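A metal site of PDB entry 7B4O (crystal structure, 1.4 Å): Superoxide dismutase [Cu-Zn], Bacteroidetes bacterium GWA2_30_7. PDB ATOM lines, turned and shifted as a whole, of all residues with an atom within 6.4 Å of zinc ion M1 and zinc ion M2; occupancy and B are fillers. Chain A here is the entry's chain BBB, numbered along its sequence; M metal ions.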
ATOM      1  N   GLY A  49     -24.646  -2.362   2.464  1.00  0.00           N
ATOM      2  CA  GLY A  49     -23.294  -2.310   3.016  1.00  0.00           C
ATOM      3  C   GLY A  49     -22.418  -3.394   2.405  1.00  0.00           C
ATOM      4  O   GLY A  49     -22.870  -4.546   2.262  1.00  0.00           O
ATOM      5  N   PHE A  50     -21.195  -3.026   2.056  1.00  0.00           N
ATOM      6  CA  PHE A  50     -20.262  -3.844   1.256  1.00  0.00           C
ATOM      7  C   PHE A  50     -18.886  -3.726   1.933  1.00  0.00           C
ATOM      8  O   PHE A  50     -18.237  -2.663   1.783  1.00  0.00           O
ATOM      9  CB  PHE A  50     -20.285  -3.316  -0.169  1.00  0.00           C
ATOM     10  CG  PHE A  50     -19.433  -4.068  -1.176  1.00  0.00           C
ATOM     11  CD1 PHE A  50     -19.847  -5.294  -1.665  1.00  0.00           C
ATOM     12  CD2 PHE A  50     -18.244  -3.530  -1.638  1.00  0.00           C
ATOM     13  CE1 PHE A  50     -19.072  -5.980  -2.580  1.00  0.00           C
ATOM     14  CE2 PHE A  50     -17.469  -4.224  -2.546  1.00  0.00           C
ATOM     15  CZ  PHE A  50     -17.893  -5.444  -3.027  1.00  0.00           C
ATOM     16  N   HIS A  51     -18.496  -4.734   2.698  1.00  0.00           N
ATOM     17  CA  HIS A  51     -17.372  -4.585   3.652  1.00  0.00           C
ATOM     18  C   HIS A  51     -16.424  -5.780   3.655  1.00  0.00           C
ATOM     19  O   HIS A  51     -16.874  -6.907   3.444  1.00  0.00           O
ATOM     20  CB  HIS A  51     -17.873  -4.451   5.087  1.00  0.00           C
ATOM     21  CG  HIS A  51     -18.841  -3.349   5.291  1.00  0.00           C
ATOM     22  ND1 HIS A  51     -19.903  -3.510   6.139  1.00  0.00           N
ATOM     23  CD2 HIS A  51     -18.923  -2.097   4.776  1.00  0.00           C
ATOM     24  CE1 HIS A  51     -20.595  -2.384   6.161  1.00  0.00           C
ATOM     25  NE2 HIS A  51     -20.023  -1.502   5.339  1.00  0.00           N
ATOM     26  N   ILE A  52     -15.170  -5.508   3.986  1.00  0.00           N
ATOM     27  CA  ILE A  52     -14.205  -6.559   4.368  1.00  0.00           C
ATOM     28  C   ILE A  52     -14.280  -6.696   5.883  1.00  0.00           C
ATOM     29  O   ILE A  52     -14.060  -5.689   6.607  1.00  0.00           O
ATOM     30  CB  ILE A  52     -12.774  -6.236   3.904  1.00  0.00           C
ATOM     31  CG1 ILE A  52     -12.731  -5.891   2.412  1.00  0.00           C
ATOM     32  CG2 ILE A  52     -11.838  -7.395   4.256  1.00  0.00           C
ATOM     33  CD1 ILE A  52     -11.379  -5.566   1.888  1.00  0.00           C
ATOM     34  N   HIS A  53     -14.584  -7.888   6.360  1.00  0.00           N
ATOM     35  CA  HIS A  53     -14.634  -8.204   7.807  1.00  0.00           C
ATOM     36  C   HIS A  53     -13.350  -8.940   8.200  1.00  0.00           C
ATOM     37  O   HIS A  53     -12.597  -9.422   7.322  1.00  0.00           O
ATOM     38  CB  HIS A  53     -15.930  -8.939   8.158  1.00  0.00           C
ATOM     39  CG  HIS A  53     -17.128  -8.063   8.230  1.00  0.00           C
ATOM     40  ND1 HIS A  53     -17.947  -8.060   9.330  1.00  0.00           N
ATOM     41  CD2 HIS A  53     -17.657  -7.169   7.344  1.00  0.00           C
ATOM     42  CE1 HIS A  53     -18.965  -7.249   9.104  1.00  0.00           C
ATOM     43  NE2 HIS A  53     -18.794  -6.649   7.902  1.00  0.00           N
ATOM     44  N   GLY A  68     -16.060  -8.441  13.193  1.00  0.00           N
ATOM     45  CA  GLY A  68     -16.280  -7.023  12.899  1.00  0.00           C
ATOM     46  C   GLY A  68     -15.550  -6.593  11.645  1.00  0.00           C
ATOM     47  O   GLY A  68     -15.023  -7.449  10.907  1.00  0.00           O
ATOM     48  N   HIS A  69     -15.521  -5.296  11.390  1.00  0.00           N
ATOM     49  CA  HIS A  69     -14.851  -4.747  10.188  1.00  0.00           C
ATOM     50  C   HIS A  69     -13.347  -4.972  10.289  1.00  0.00           C
ATOM     51  O   HIS A  69     -12.784  -4.898  11.402  1.00  0.00           O
ATOM     52  CB  HIS A  69     -15.241  -3.300   9.993  1.00  0.00           C
ATOM     53  CG  HIS A  69     -16.650  -3.188   9.534  1.00  0.00           C
ATOM     54  ND1 HIS A  69     -17.201  -1.999   9.141  1.00  0.00           N
ATOM     55  CD2 HIS A  69     -17.586  -4.130   9.372  1.00  0.00           C
ATOM     56  CE1 HIS A  69     -18.449  -2.198   8.792  1.00  0.00           C
ATOM     57  NE2 HIS A  69     -18.708  -3.516   8.887  1.00  0.00           N
ATOM     58  N   PHE A  70     -12.723  -5.255   9.158  1.00  0.00           N
ATOM     59  CA  PHE A  70     -11.256  -5.372   9.082  1.00  0.00           C
ATOM     60  C   PHE A  70     -10.676  -3.995   9.375  1.00  0.00           C
ATOM     61  O   PHE A  70     -10.901  -3.051   8.598  1.00  0.00           O
ATOM     62  CB  PHE A  70     -10.816  -5.945   7.739  1.00  0.00           C
ATOM     63  CG  PHE A  70      -9.335  -6.131   7.638  1.00  0.00           C
ATOM     64  CD1 PHE A  70      -8.613  -6.763   8.632  1.00  0.00           C
ATOM     65  CD2 PHE A  70      -8.664  -5.665   6.509  1.00  0.00           C
ATOM     66  CE1 PHE A  70      -7.242  -6.944   8.508  1.00  0.00           C
ATOM     67  CE2 PHE A  70      -7.292  -5.839   6.393  1.00  0.00           C
ATOM     68  CZ  PHE A  70      -6.590  -6.470   7.386  1.00  0.00           C
ATOM     69  N   SER A  76     -12.082   4.593  13.180  1.00  0.00           N
ATOM     70  CA  SER A  76     -13.565   4.633  13.202  1.00  0.00           C
ATOM     71  C   SER A  76     -14.101   4.137  11.865  1.00  0.00           C
ATOM     72  O   SER A  76     -13.360   4.171  10.854  1.00  0.00           O
ATOM     73  CB  SER A  76     -14.057   6.017  13.496  1.00  0.00           C
ATOM     74  OG  SER A  76     -13.630   6.400  14.786  1.00  0.00           O
ATOM     75  N   HIS A  77     -15.371   3.747  11.859  1.00  0.00           N
ATOM     76  CA  HIS A  77     -16.109   3.376  10.627  1.00  0.00           C
ATOM     77  C   HIS A  77     -16.355   4.644   9.810  1.00  0.00           C
ATOM     78  O   HIS A  77     -16.734   5.673  10.399  1.00  0.00           O
ATOM     79  CB  HIS A  77     -17.431   2.685  10.984  1.00  0.00           C
ATOM     80  CG  HIS A  77     -18.190   2.308   9.758  1.00  0.00           C
ATOM     81  ND1 HIS A  77     -17.824   1.222   8.975  1.00  0.00           N
ATOM     82  CD2 HIS A  77     -19.233   2.903   9.158  1.00  0.00           C
ATOM     83  CE1 HIS A  77     -18.658   1.157   7.956  1.00  0.00           C
ATOM     84  NE2 HIS A  77     -19.521   2.188   8.045  1.00  0.00           N
ATOM     85  N   GLY A  78     -16.184   4.551   8.487  1.00  0.00           N
ATOM     86  CA  GLY A  78     -16.471   5.676   7.591  1.00  0.00           C
ATOM     87  C   GLY A  78     -16.712   5.225   6.168  1.00  0.00           C
ATOM     88  O   GLY A  78     -16.947   4.016   5.944  1.00  0.00           O
ATOM     89  N   ARG A  85     -11.554   5.770   8.326  1.00  0.00           N
ATOM     90  CA  ARG A  85     -12.306   4.582   7.876  1.00  0.00           C
ATOM     91  C   ARG A  85     -11.551   3.330   8.331  1.00  0.00           C
ATOM     92  O   ARG A  85     -10.335   3.383   8.565  1.00  0.00           O
ATOM     93  CB  ARG A  85     -12.475   4.576   6.356  1.00  0.00           C
ATOM     94  CG  ARG A  85     -11.175   4.493   5.565  1.00  0.00           C
ATOM     95  CD  ARG A  85     -11.400   4.213   4.089  1.00  0.00           C
ATOM     96  NE  ARG A  85     -11.310   2.799   3.751  1.00  0.00           N
ATOM     97  CZ  ARG A  85     -11.146   2.298   2.518  1.00  0.00           C
ATOM     98  NH1 ARG A  85     -11.048   3.111   1.473  1.00  0.00           N
ATOM     99  NH2 ARG A  85     -11.050   0.995   2.346  1.00  0.00           N
ATOM    100  N   HIS A  86     -12.283   2.228   8.401  1.00  0.00           N
ATOM    101  CA  HIS A  86     -11.703   0.869   8.471  1.00  0.00           C
ATOM    102  C   HIS A  86     -11.111   0.524   7.101  1.00  0.00           C
ATOM    103  O   HIS A  86     -11.689   0.967   6.091  1.00  0.00           O
ATOM    104  CB  HIS A  86     -12.783  -0.130   8.883  1.00  0.00           C
ATOM    105  CG  HIS A  86     -13.437   0.172  10.188  1.00  0.00           C
ATOM    106  ND1 HIS A  86     -14.789  -0.085  10.399  1.00  0.00           N
ATOM    107  CD2 HIS A  86     -12.956   0.694  11.334  1.00  0.00           C
ATOM    108  CE1 HIS A  86     -15.090   0.239  11.645  1.00  0.00           C
ATOM    109  NE2 HIS A  86     -13.980   0.730  12.233  1.00  0.00           N
ATOM    110  N   GLY A  88     -11.594  -2.159   5.827  1.00  0.00           N
ATOM    111  CA  GLY A  88     -12.717  -2.910   5.259  1.00  0.00           C
ATOM    112  C   GLY A  88     -13.900  -2.064   4.791  1.00  0.00           C
ATOM    113  O   GLY A  88     -14.871  -2.674   4.347  1.00  0.00           O
ATOM    114  N   ASP A  89     -13.853  -0.743   4.905  1.00  0.00           N
ATOM    115  CA  ASP A  89     -15.037   0.115   4.603  1.00  0.00           C
ATOM    116  C   ASP A  89     -15.100   0.399   3.099  1.00  0.00           C
ATOM    117  O   ASP A  89     -14.617   1.460   2.672  1.00  0.00           O
ATOM    118  CB  ASP A  89     -15.016   1.389   5.438  1.00  0.00           C
ATOM    119  CG  ASP A  89     -15.292   1.125   6.908  1.00  0.00           C
ATOM    120  OD1 ASP A  89     -15.738   0.005   7.227  1.00  0.00           O
ATOM    121  OD2 ASP A  89     -15.032   2.029   7.732  1.00  0.00           O
ATOM    122  N   ILE A 124     -18.394  -9.312   3.426  1.00  0.00           N
ATOM    123  CA  ILE A 124     -19.785  -9.402   3.939  1.00  0.00           C
ATOM    124  C   ILE A 124     -20.607  -8.396   3.147  1.00  0.00           C
ATOM    125  O   ILE A 124     -20.190  -7.236   3.012  1.00  0.00           O
ATOM    126  CB  ILE A 124     -19.843  -9.125   5.457  1.00  0.00           C
ATOM    127  CG1 ILE A 124     -19.171 -10.236   6.272  1.00  0.00           C
ATOM    128  CG2 ILE A 124     -21.275  -8.906   5.892  1.00  0.00           C
ATOM    129  CD1 ILE A 124     -19.901 -11.554   6.254  1.00  0.00           C
ATOM    130  N   HIS A 126     -24.363  -6.675   3.435  1.00  0.00           N
ATOM    131  CA  HIS A 126     -25.350  -6.416   4.503  1.00  0.00           C
ATOM    132  C   HIS A 126     -26.754  -6.265   3.914  1.00  0.00           C
ATOM    133  O   HIS A 126     -26.916  -5.924   2.722  1.00  0.00           O
ATOM    134  CB  HIS A 126     -24.941  -5.193   5.306  1.00  0.00           C
ATOM    135  CG  HIS A 126     -23.800  -5.427   6.218  1.00  0.00           C
ATOM    136  ND1 HIS A 126     -23.939  -5.979   7.471  1.00  0.00           N
ATOM    137  CD2 HIS A 126     -22.492  -5.188   6.060  1.00  0.00           C
ATOM    138  CE1 HIS A 126     -22.760  -6.060   8.057  1.00  0.00           C
ATOM    139  NE2 HIS A 126     -21.847  -5.537   7.221  1.00  0.00           N
ATOM    140  N   ASP A 130     -25.140   0.957   4.389  1.00  0.00           N
ATOM    141  CA  ASP A 130     -24.138   1.538   5.301  1.00  0.00           C
ATOM    142  C   ASP A 130     -24.333   3.060   5.265  1.00  0.00           C
ATOM    143  O   ASP A 130     -24.155   3.634   4.181  1.00  0.00           O
ATOM    144  CB  ASP A 130     -22.755   1.091   4.838  1.00  0.00           C
ATOM    145  CG  ASP A 130     -21.605   1.618   5.647  1.00  0.00           C
ATOM    146  OD1 ASP A 130     -21.816   2.539   6.482  1.00  0.00           O
ATOM    147  OD2 ASP A 130     -20.493   1.104   5.410  1.00  0.00           O
ATOM    148  N   PRO A 136     -20.364   0.898  15.169  1.00  0.00           N
ATOM    149  CA  PRO A 136     -19.116   0.691  14.423  1.00  0.00           C
ATOM    150  C   PRO A 136     -19.238   0.107  13.006  1.00  0.00           C
ATOM    151  O   PRO A 136     -18.205  -0.226  12.414  1.00  0.00           O
ATOM    152  CB  PRO A 136     -18.441  -0.372  15.303  1.00  0.00           C
ATOM    153  CG  PRO A 136     -19.600  -1.244  15.773  1.00  0.00           C
ATOM    154  CD  PRO A 136     -20.794  -0.317  15.882  1.00  0.00           C
ATOM    155  N   THR A 137     -20.458  -0.031  12.473  1.00  0.00           N
ATOM    156  CA  THR A 137     -20.736  -0.775  11.207  1.00  0.00           C
ATOM    157  C   THR A 137     -21.519   0.074  10.193  1.00  0.00           C
ATOM    158  O   THR A 137     -21.790  -0.432   9.112  1.00  0.00           O
ATOM    159  CB  THR A 137     -21.499  -2.075  11.477  1.00  0.00           C
ATOM    160  OG1 THR A 137     -22.870  -1.755  11.721  1.00  0.00           O
ATOM    161  CG2 THR A 137     -20.924  -2.868  12.622  1.00  0.00           C
ATOM    162  N   GLY A 138     -21.906   1.308  10.518  1.00  0.00           N
ATOM    163  CA  GLY A 138     -22.742   2.141   9.644  1.00  0.00           C
ATOM    164  C   GLY A 138     -24.196   1.717   9.685  1.00  0.00           C
ATOM    165  O   GLY A 138     -24.953   2.079   8.744  1.00  0.00           O
ATOM    166  N   ALA A 140     -25.608  -1.129   9.141  1.00  0.00           N
ATOM    167  CA  ALA A 140     -25.945  -1.855   7.891  1.00  0.00           C
ATOM    168  C   ALA A 140     -26.709  -3.150   8.218  1.00  0.00           C
ATOM    169  O   ALA A 140     -27.203  -3.773   7.285  1.00  0.00           O
ATOM    170  CB  ALA A 140     -24.722  -2.118   7.050  1.00  0.00           C
ATOM    171  N   ARG A 143     -26.251  -9.756   7.940  1.00  0.00           N
ATOM    172  CA  ARG A 143     -25.315 -10.229   6.897  1.00  0.00           C
ATOM    173  C   ARG A 143     -26.085 -11.137   5.965  1.00  0.00           C
ATOM    174  O   ARG A 143     -26.624 -12.143   6.441  1.00  0.00           O
ATOM    175  CB  ARG A 143     -24.143 -10.941   7.577  1.00  0.00           C
ATOM    176  CG  ARG A 143     -23.498 -10.063   8.636  1.00  0.00           C
ATOM    177  CD  ARG A 143     -22.447 -10.756   9.459  1.00  0.00           C
ATOM    178  NE  ARG A 143     -22.014  -9.792  10.453  1.00  0.00           N
ATOM    179  CZ  ARG A 143     -20.846  -9.766  11.047  1.00  0.00           C
ATOM    180  NH1 ARG A 143     -19.929 -10.673  10.762  1.00  0.00           N
ATOM    181  NH2 ARG A 143     -20.581  -8.797  11.909  1.00  0.00           N
HETATM  182 ZN    ZN M   1     -19.936  -4.878   7.605  1.00  0.00          ZN
HETATM  183 ZN    ZN M   2     -16.396  -0.193   9.067  1.00  0.00          ZN
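Merely in contact with zinc ion M2: Pro 136 (3.8 Å).
OD1 of Asp 89 is bound to zinc ion M2. ND1 of His 69 binds zinc ion M2. Zinc ion M2 is bound by ND1 of His 77 (2.0 Å). A ring nitrogen (ND1) of His 86 binds zinc ion M2 (2.1 Å).
The side-chain carboxylate (OD2) of Asp 89 is in hydrogen-bond range of the backbone NH (N) of Gly 78 (2.9 Å). The backbone NH (N) of Ile 124 lies within hydrogen-bond range of the backbone carbonyl oxygen (O) of His 51 (2.8 Å). A ring nitrogen (NE2) of His 77 is in hydrogen-bond range of the side-chain carboxylate of Asp 130, at 2.8 Å. The backbone carbonyl oxygen (O) of Gly 49 lies within hydrogen-bond range of the backbone NH (N) of His 126, 2.9 Å away. The backbone NH of His 86 lies within hydrogen-bond range of the backbone carbonyl oxygen of Ser 76 (3.3 Å). OD2 of Asp 130 sits at hydrogen-bond distance from NE2 of His 51, at 2.6 Å. The backbone carbonyl oxygen of Gly 68 lies close to a ring nitrogen (ND1) of His 53 (3.4 Å).
Zinc ion M1 is bound by a ring nitrogen (ND1) of His 51 (2.0 Å). A ring nitrogen (NE2) of His 126 binds zinc ion M1, at 2.1 Å. Zinc ion M1 is bound by NE2 of His 53. NE2 of His 69 binds zinc ion M1 (2.2 Å). Zinc ion M1 has four donor atoms within binding distance.
Within 4 Å of zinc ion M1: His 51, His 53, His 69 and His 126. The nearest printed residue that does not touch zinc ion M1 is Ile 124 (4.6 Å).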
